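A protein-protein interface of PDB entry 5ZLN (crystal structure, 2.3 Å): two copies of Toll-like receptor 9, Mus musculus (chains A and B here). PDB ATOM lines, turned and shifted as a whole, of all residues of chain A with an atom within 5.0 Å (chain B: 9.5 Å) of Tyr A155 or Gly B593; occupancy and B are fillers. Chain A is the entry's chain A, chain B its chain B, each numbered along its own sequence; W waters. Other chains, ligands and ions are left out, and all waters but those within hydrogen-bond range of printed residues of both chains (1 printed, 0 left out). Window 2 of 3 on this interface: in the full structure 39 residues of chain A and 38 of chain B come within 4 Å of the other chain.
The side-chain amino group (NZ) of Lys A156 is in salt-bridge range of the side-chain carboxylate (OD1) of Asp B591, 3.2 Å away.
NE of Arg B588 lies within salt-bridge range of OE1 of Glu B592 (3.7 Å).
The side-chain hydroxyl of Tyr A155 lies within hydrogen-bond range of the side-chain amide nitrogen of Asn A238 (3.5 Å).
Among the printed residues, merely in contact across the chains: Tyr A155 with Glu B592 (3.6 Å), Tyr A155 with Gly B593 (3.996 Å), Asn A238 with Glu B592 (3.7 Å) and Pro A239 with Glu B592 (3.6 Å).
Printed residues of chain B within 4 Å of Tyr A155: Glu B592 (3.6 Å) and Gly B593 (3.996 Å).
Of the printed residues of chain B, Asn A238 touches Glu B592.
Of chain B, only Glu B592 (3.6 Å) comes within 4 Å of Pro A239.
Printed residues of chain A within 4 Å of Glu B592: Tyr A155 (3.6 Å), Asn A238 (3.7 Å) and Pro A239 (3.6 Å).
Printed residues of chain A within 4 Å of Gly B593: Tyr A155.
The nearest printed residue of chain A that does not touch Gly B593 is Pro A239 (4.7 Å).
The nearest printed residue of chain B that does not touch Asn A238 is Leu B595 (4.3 Å).
Printed residues of chain B that touch a printed residue of chain A: Asp B591, Glu B592 and Gly B593.
Of the 8 printed residues of chain A, 4 touch a printed residue of chain B.
Hydrophobic or aromatic side chains of chain A within 4 Å of the printed part of chain B: Tyr A155 and Pro A239.
No position is printed for both chains.
Water W1 lies within hydrogen-bond range of N of Gly B593, O of Asp B591 and NZ of Lys A156.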
ATOM      1  N   CYS A 153     -14.370 -31.230 -40.370  1.00  0.00           N
ATOM      2  CA  CYS A 153     -12.940 -30.839 -40.374  1.00  0.00           C
ATOM      3  C   CYS A 153     -12.683 -29.537 -39.638  1.00  0.00           C
ATOM      4  O   CYS A 153     -12.517 -28.469 -40.239  1.00  0.00           O
ATOM      5  CB  CYS A 153     -12.363 -30.775 -41.795  1.00  0.00           C
ATOM      6  SG  CYS A 153     -10.558 -30.545 -41.788  1.00  0.00           S
ATOM      7  N   TYR A 154     -12.657 -29.658 -38.318  1.00  0.00           N
ATOM      8  CA  TYR A 154     -12.360 -28.561 -37.429  1.00  0.00           C
ATOM      9  C   TYR A 154     -11.742 -29.075 -36.137  1.00  0.00           C
ATOM     10  O   TYR A 154     -11.551 -30.274 -35.987  1.00  0.00           O
ATOM     11  CB  TYR A 154     -13.616 -27.727 -37.189  1.00  0.00           C
ATOM     12  CG  TYR A 154     -14.613 -28.288 -36.197  1.00  0.00           C
ATOM     13  CD1 TYR A 154     -15.174 -29.537 -36.374  1.00  0.00           C
ATOM     14  CD2 TYR A 154     -15.054 -27.522 -35.114  1.00  0.00           C
ATOM     15  CE1 TYR A 154     -16.093 -30.025 -35.489  1.00  0.00           C
ATOM     16  CE2 TYR A 154     -15.988 -28.022 -34.214  1.00  0.00           C
ATOM     17  CZ  TYR A 154     -16.514 -29.270 -34.420  1.00  0.00           C
ATOM     18  OH  TYR A 154     -17.439 -29.797 -33.552  1.00  0.00           O
ATOM     19  N   TYR A 155     -11.407 -28.182 -35.212  1.00  0.00           N
ATOM     20  CA  TYR A 155     -10.550 -28.570 -34.042  1.00  0.00           C
ATOM     21  C   TYR A 155     -11.119 -29.723 -33.179  1.00  0.00           C
ATOM     22  O   TYR A 155     -10.376 -30.460 -32.559  1.00  0.00           O
ATOM     23  CB  TYR A 155     -10.271 -27.354 -33.152  1.00  0.00           C
ATOM     24  CG  TYR A 155     -11.497 -26.843 -32.420  1.00  0.00           C
ATOM     25  CD1 TYR A 155     -12.348 -25.899 -33.007  1.00  0.00           C
ATOM     26  CD2 TYR A 155     -11.812 -27.313 -31.149  1.00  0.00           C
ATOM     27  CE1 TYR A 155     -13.462 -25.441 -32.343  1.00  0.00           C
ATOM     28  CE2 TYR A 155     -12.934 -26.871 -30.486  1.00  0.00           C
ATOM     29  CZ  TYR A 155     -13.753 -25.927 -31.096  1.00  0.00           C
ATOM     30  OH  TYR A 155     -14.848 -25.447 -30.430  1.00  0.00           O
ATOM     31  N   LYS A 156     -12.442 -29.869 -33.146  1.00  0.00           N
ATOM     32  CA  LYS A 156     -13.043 -30.900 -32.322  1.00  0.00           C
ATOM     33  C   LYS A 156     -13.179 -32.219 -33.074  1.00  0.00           C
ATOM     34  O   LYS A 156     -13.416 -33.242 -32.453  1.00  0.00           O
ATOM     35  CB  LYS A 156     -14.410 -30.430 -31.834  1.00  0.00           C
ATOM     36  CG  LYS A 156     -14.671 -30.691 -30.382  1.00  0.00           C
ATOM     37  CD  LYS A 156     -15.739 -29.722 -29.829  1.00  0.00           C
ATOM     38  CE  LYS A 156     -15.880 -29.835 -28.317  1.00  0.00           C
ATOM     39  NZ  LYS A 156     -15.680 -31.232 -27.786  1.00  0.00           N
ATOM     40  N   ASN A 157     -13.080 -32.172 -34.403  1.00  0.00           N
ATOM     41  CA  ASN A 157     -13.154 -33.363 -35.260  1.00  0.00           C
ATOM     42  C   ASN A 157     -12.216 -33.094 -36.448  1.00  0.00           C
ATOM     43  O   ASN A 157     -12.667 -32.781 -37.537  1.00  0.00           O
ATOM     44  CB  ASN A 157     -14.593 -33.574 -35.729  1.00  0.00           C
ATOM     45  CG  ASN A 157     -14.783 -34.874 -36.541  1.00  0.00           C
ATOM     46  OD1 ASN A 157     -14.096 -35.857 -36.330  1.00  0.00           O
ATOM     47  ND2 ASN A 157     -15.771 -34.876 -37.441  1.00  0.00           N
ATOM     48  N   PRO A 158     -10.909 -33.157 -36.217  1.00  0.00           N
ATOM     49  CA  PRO A 158      -9.930 -32.631 -37.176  1.00  0.00           C
ATOM     50  C   PRO A 158      -9.719 -33.483 -38.394  1.00  0.00           C
ATOM     51  O   PRO A 158      -9.937 -34.681 -38.350  1.00  0.00           O
ATOM     52  CB  PRO A 158      -8.602 -32.577 -36.369  1.00  0.00           C
ATOM     53  CG  PRO A 158      -8.831 -33.373 -35.152  1.00  0.00           C
ATOM     54  CD  PRO A 158     -10.286 -33.699 -35.000  1.00  0.00           C
ATOM     55  N   ASN A 238     -12.821 -20.331 -28.354  1.00  0.00           N
ATOM     56  CA  ASN A 238     -12.486 -21.678 -28.756  1.00  0.00           C
ATOM     57  C   ASN A 238     -11.280 -21.532 -29.659  1.00  0.00           C
ATOM     58  O   ASN A 238     -10.923 -20.403 -30.009  1.00  0.00           O
ATOM     59  CB  ASN A 238     -13.686 -22.285 -29.507  1.00  0.00           C
ATOM     60  CG  ASN A 238     -14.069 -21.505 -30.802  1.00  0.00           C
ATOM     61  OD1 ASN A 238     -13.732 -20.307 -31.003  1.00  0.00           O
ATOM     62  ND2 ASN A 238     -14.746 -22.214 -31.714  1.00  0.00           N
ATOM     63  N   PRO A 239     -10.616 -22.646 -30.034  1.00  0.00           N
ATOM     64  CA  PRO A 239      -9.505 -22.492 -30.971  1.00  0.00           C
ATOM     65  C   PRO A 239      -9.973 -21.824 -32.258  1.00  0.00           C
ATOM     66  O   PRO A 239     -11.091 -22.083 -32.755  1.00  0.00           O
ATOM     67  CB  PRO A 239      -9.058 -23.921 -31.231  1.00  0.00           C
ATOM     68  CG  PRO A 239      -9.369 -24.604 -29.950  1.00  0.00           C
ATOM     69  CD  PRO A 239     -10.684 -24.005 -29.502  1.00  0.00           C
ATOM     70  N   MET B 586     -13.724 -26.163 -15.197  1.00  0.00           N
ATOM     71  CA  MET B 586     -12.610 -26.823 -15.872  1.00  0.00           C
ATOM     72  C   MET B 586     -13.143 -27.896 -16.811  1.00  0.00           C
ATOM     73  O   MET B 586     -12.558 -28.187 -17.846  1.00  0.00           O
ATOM     74  CB  MET B 586     -11.622 -27.440 -14.859  1.00  0.00           C
ATOM     75  CG  MET B 586     -10.231 -27.619 -15.436  1.00  0.00           C
ATOM     76  SD  MET B 586      -9.483 -26.000 -15.722  1.00  0.00           S
ATOM     77  CE  MET B 586      -8.647 -26.378 -17.233  1.00  0.00           C
ATOM     78  N   GLY B 587     -14.265 -28.485 -16.450  1.00  0.00           N
ATOM     79  CA  GLY B 587     -14.937 -29.418 -17.344  1.00  0.00           C
ATOM     80  C   GLY B 587     -15.125 -28.791 -18.709  1.00  0.00           C
ATOM     81  O   GLY B 587     -14.757 -29.379 -19.736  1.00  0.00           O
ATOM     82  N   ARG B 588     -15.682 -27.597 -18.723  1.00  0.00           N
ATOM     83  CA  ARG B 588     -15.915 -26.934 -19.989  1.00  0.00           C
ATOM     84  C   ARG B 588     -14.591 -26.487 -20.639  1.00  0.00           C
ATOM     85  O   ARG B 588     -14.437 -26.573 -21.857  1.00  0.00           O
ATOM     86  CB  ARG B 588     -16.903 -25.790 -19.826  1.00  0.00           C
ATOM     87  CG  ARG B 588     -16.924 -24.787 -20.964  1.00  0.00           C
ATOM     88  CD  ARG B 588     -17.845 -25.097 -22.142  1.00  0.00           C
ATOM     89  NE  ARG B 588     -18.256 -23.803 -22.693  1.00  0.00           N
ATOM     90  CZ  ARG B 588     -19.137 -22.968 -22.114  1.00  0.00           C
ATOM     91  NH1 ARG B 588     -19.415 -21.790 -22.690  1.00  0.00           N
ATOM     92  NH2 ARG B 588     -19.754 -23.302 -20.973  1.00  0.00           N
ATOM     93  N   MET B 589     -13.620 -26.062 -19.830  1.00  0.00           N
ATOM     94  CA  MET B 589     -12.360 -25.634 -20.377  1.00  0.00           C
ATOM     95  C   MET B 589     -11.604 -26.780 -21.079  1.00  0.00           C
ATOM     96  O   MET B 589     -11.031 -26.589 -22.145  1.00  0.00           O
ATOM     97  CB  MET B 589     -11.539 -24.971 -19.298  1.00  0.00           C
ATOM     98  CG  MET B 589     -12.110 -23.614 -18.879  1.00  0.00           C
ATOM     99  SD  MET B 589     -11.418 -22.908 -17.356  1.00  0.00           S
ATOM    100  CE  MET B 589      -9.757 -22.602 -17.906  1.00  0.00           C
ATOM    101  N   TRP B 590     -11.641 -27.976 -20.485  1.00  0.00           N
ATOM    102  CA  TRP B 590     -10.965 -29.139 -21.032  1.00  0.00           C
ATOM    103  C   TRP B 590     -11.776 -29.830 -22.126  1.00  0.00           C
ATOM    104  O   TRP B 590     -11.343 -30.839 -22.677  1.00  0.00           O
ATOM    105  CB  TRP B 590     -10.631 -30.102 -19.897  1.00  0.00           C
ATOM    106  CG  TRP B 590      -9.419 -29.739 -19.160  1.00  0.00           C
ATOM    107  CD1 TRP B 590      -8.435 -28.896 -19.584  1.00  0.00           C
ATOM    108  CD2 TRP B 590      -9.011 -30.227 -17.879  1.00  0.00           C
ATOM    109  NE1 TRP B 590      -7.457 -28.821 -18.646  1.00  0.00           N
ATOM    110  CE2 TRP B 590      -7.776 -29.632 -17.590  1.00  0.00           C
ATOM    111  CE3 TRP B 590      -9.580 -31.100 -16.947  1.00  0.00           C
ATOM    112  CZ2 TRP B 590      -7.077 -29.889 -16.423  1.00  0.00           C
ATOM    113  CZ3 TRP B 590      -8.898 -31.351 -15.765  1.00  0.00           C
ATOM    114  CH2 TRP B 590      -7.656 -30.734 -15.509  1.00  0.00           C
ATOM    115  N   ASP B 591     -12.945 -29.279 -22.451  1.00  0.00           N
ATOM    116  CA  ASP B 591     -13.691 -29.683 -23.632  1.00  0.00           C
ATOM    117  C   ASP B 591     -13.489 -28.739 -24.821  1.00  0.00           C
ATOM    118  O   ASP B 591     -14.118 -28.932 -25.838  1.00  0.00           O
ATOM    119  CB  ASP B 591     -15.173 -29.777 -23.307  1.00  0.00           C
ATOM    120  CG  ASP B 591     -15.861 -30.863 -24.090  1.00  0.00           C
ATOM    121  OD1 ASP B 591     -16.814 -30.546 -24.844  1.00  0.00           O
ATOM    122  OD2 ASP B 591     -15.424 -32.038 -24.001  1.00  0.00           O
ATOM    123  N   GLU B 592     -12.596 -27.754 -24.715  1.00  0.00           N
ATOM    124  CA  GLU B 592     -12.337 -26.821 -25.814  1.00  0.00           C
ATOM    125  C   GLU B 592     -11.103 -27.159 -26.647  1.00  0.00           C
ATOM    126  O   GLU B 592     -10.181 -26.344 -26.768  1.00  0.00           O
ATOM    127  CB  GLU B 592     -12.158 -25.383 -25.304  1.00  0.00           C
ATOM    128  CG  GLU B 592     -13.377 -24.682 -24.760  1.00  0.00           C
ATOM    129  CD  GLU B 592     -14.518 -24.511 -25.744  1.00  0.00           C
ATOM    130  OE1 GLU B 592     -15.571 -24.059 -25.236  1.00  0.00           O
ATOM    131  OE2 GLU B 592     -14.403 -24.825 -26.961  1.00  0.00           O
ATOM    132  N   GLY B 593     -11.081 -28.339 -27.250  1.00  0.00           N
ATOM    133  CA  GLY B 593      -9.902 -28.794 -27.967  1.00  0.00           C
ATOM    134  C   GLY B 593      -8.697 -28.711 -27.035  1.00  0.00           C
ATOM    135  O   GLY B 593      -8.781 -28.988 -25.842  1.00  0.00           O
ATOM    136  N   GLY B 594      -7.573 -28.285 -27.550  1.00  0.00           N
ATOM    137  CA  GLY B 594      -6.405 -28.235 -26.694  1.00  0.00           C
ATOM    138  C   GLY B 594      -6.186 -26.927 -25.975  1.00  0.00           C
ATOM    139  O   GLY B 594      -5.179 -26.752 -25.349  1.00  0.00           O
ATOM    140  N   LEU B 595      -7.143 -26.025 -26.022  1.00  0.00           N
ATOM    141  CA  LEU B 595      -6.881 -24.669 -25.573  1.00  0.00           C
ATOM    142  C   LEU B 595      -6.381 -24.571 -24.148  1.00  0.00           C
ATOM    143  O   LEU B 595      -5.475 -23.795 -23.888  1.00  0.00           O
ATOM    144  CB  LEU B 595      -8.135 -23.821 -25.733  1.00  0.00           C
ATOM    145  CG  LEU B 595      -7.982 -22.333 -25.565  1.00  0.00           C
ATOM    146  CD1 LEU B 595      -6.844 -21.781 -26.442  1.00  0.00           C
ATOM    147  CD2 LEU B 595      -9.335 -21.665 -25.869  1.00  0.00           C
ATOM    148  N   TYR B 596      -6.969 -25.349 -23.226  1.00  0.00           N
ATOM    149  CA  TYR B 596      -6.627 -25.227 -21.806  1.00  0.00           C
ATOM    150  C   TYR B 596      -5.942 -26.487 -21.301  1.00  0.00           C
ATOM    151  O   TYR B 596      -5.915 -26.778 -20.106  1.00  0.00           O
ATOM    152  CB  TYR B 596      -7.864 -24.899 -20.972  1.00  0.00           C
ATOM    153  CG  TYR B 596      -8.498 -23.603 -21.352  1.00  0.00           C
ATOM    154  CD1 TYR B 596      -7.893 -22.393 -21.029  1.00  0.00           C
ATOM    155  CD2 TYR B 596      -9.698 -23.565 -22.034  1.00  0.00           C
ATOM    156  CE1 TYR B 596      -8.462 -21.180 -21.376  1.00  0.00           C
ATOM    157  CE2 TYR B 596     -10.275 -22.370 -22.407  1.00  0.00           C
ATOM    158  CZ  TYR B 596      -9.668 -21.183 -22.080  1.00  0.00           C
ATOM    159  OH  TYR B 596     -10.275 -20.027 -22.451  1.00  0.00           O
ATOM    160  N   LEU B 597      -5.344 -27.224 -22.221  1.00  0.00           N
ATOM    161  CA  LEU B 597      -4.747 -28.507 -21.873  1.00  0.00           C
ATOM    162  C   LEU B 597      -3.531 -28.364 -20.928  1.00  0.00           C
ATOM    163  O   LEU B 597      -3.250 -29.262 -20.160  1.00  0.00           O
ATOM    164  CB  LEU B 597      -4.397 -29.255 -23.155  1.00  0.00           C
ATOM    165  CG  LEU B 597      -3.653 -30.607 -23.041  1.00  0.00           C
ATOM    166  CD1 LEU B 597      -4.348 -31.637 -22.140  1.00  0.00           C
ATOM    167  CD2 LEU B 597      -3.427 -31.142 -24.462  1.00  0.00           C
ATOM    168  N   HIS B 598      -2.840 -27.223 -20.967  1.00  0.00           N
ATOM    169  CA  HIS B 598      -1.661 -26.973 -20.147  1.00  0.00           C
ATOM    170  C   HIS B 598      -1.910 -25.847 -19.168  1.00  0.00           C
ATOM    171  O   HIS B 598      -0.960 -25.193 -18.728  1.00  0.00           O
ATOM    172  CB  HIS B 598      -0.478 -26.627 -21.047  1.00  0.00           C
ATOM    173  CG  HIS B 598      -0.168 -27.690 -22.048  1.00  0.00           C
ATOM    174  ND1 HIS B 598      -0.694 -27.686 -23.318  1.00  0.00           N
ATOM    175  CD2 HIS B 598       0.560 -28.826 -21.950  1.00  0.00           C
ATOM    176  CE1 HIS B 598      -0.304 -28.772 -23.964  1.00  0.00           C
ATOM    177  NE2 HIS B 598       0.451 -29.484 -23.151  1.00  0.00           N
ATOM    178  N   ARG B 620      -9.224 -37.323 -19.040  1.00  0.00           N
ATOM    179  CA  ARG B 620      -8.234 -38.037 -19.843  1.00  0.00           C
ATOM    180  C   ARG B 620      -6.872 -38.106 -19.141  1.00  0.00           C
ATOM    181  O   ARG B 620      -6.563 -37.265 -18.281  1.00  0.00           O
ATOM    182  CB  ARG B 620      -7.992 -37.285 -21.131  1.00  0.00           C
ATOM    183  CG  ARG B 620      -9.111 -37.361 -22.144  1.00  0.00           C
ATOM    184  CD  ARG B 620      -9.020 -36.186 -23.113  1.00  0.00           C
ATOM    185  NE  ARG B 620     -10.372 -35.715 -23.254  1.00  0.00           N
ATOM    186  CZ  ARG B 620     -10.883 -34.608 -22.736  1.00  0.00           C
ATOM    187  NH1 ARG B 620     -10.139 -33.700 -22.093  1.00  0.00           N
ATOM    188  NH2 ARG B 620     -12.173 -34.401 -22.937  1.00  0.00           N
ATOM    189  N   GLN B 622      -3.966 -37.328 -20.295  1.00  0.00           N
ATOM    190  CA  GLN B 622      -3.206 -36.120 -20.634  1.00  0.00           C
ATOM    191  C   GLN B 622      -3.550 -34.997 -19.628  1.00  0.00           C
ATOM    192  O   GLN B 622      -2.674 -34.244 -19.234  1.00  0.00           O
ATOM    193  CB  GLN B 622      -3.421 -35.718 -22.117  1.00  0.00           C
ATOM    194  CG  GLN B 622      -4.919 -35.594 -22.479  1.00  0.00           C
ATOM    195  CD  GLN B 622      -5.249 -35.059 -23.892  1.00  0.00           C
ATOM    196  OE1 GLN B 622      -6.453 -34.826 -24.232  1.00  0.00           O
ATOM    197  NE2 GLN B 622      -4.205 -34.841 -24.709  1.00  0.00           N
ATOM    198  N   ASN B 623      -4.784 -34.933 -19.142  1.00  0.00           N
ATOM    199  CA  ASN B 623      -5.189 -33.882 -18.198  1.00  0.00           C
ATOM    200  C   ASN B 623      -4.439 -33.996 -16.867  1.00  0.00           C
ATOM    201  O   ASN B 623      -3.997 -32.973 -16.327  1.00  0.00           O
ATOM    202  CB  ASN B 623      -6.705 -33.899 -17.908  1.00  0.00           C
ATOM    203  CG  ASN B 623      -7.597 -33.658 -19.154  1.00  0.00           C
ATOM    204  OD1 ASN B 623      -8.698 -34.320 -19.308  1.00  0.00           O
ATOM    205  ND2 ASN B 623      -7.217 -32.672 -19.994  1.00  0.00           N
HETATM  206  O   HOH W   1     -12.622 -30.894 -27.564  1.00  0.00           O
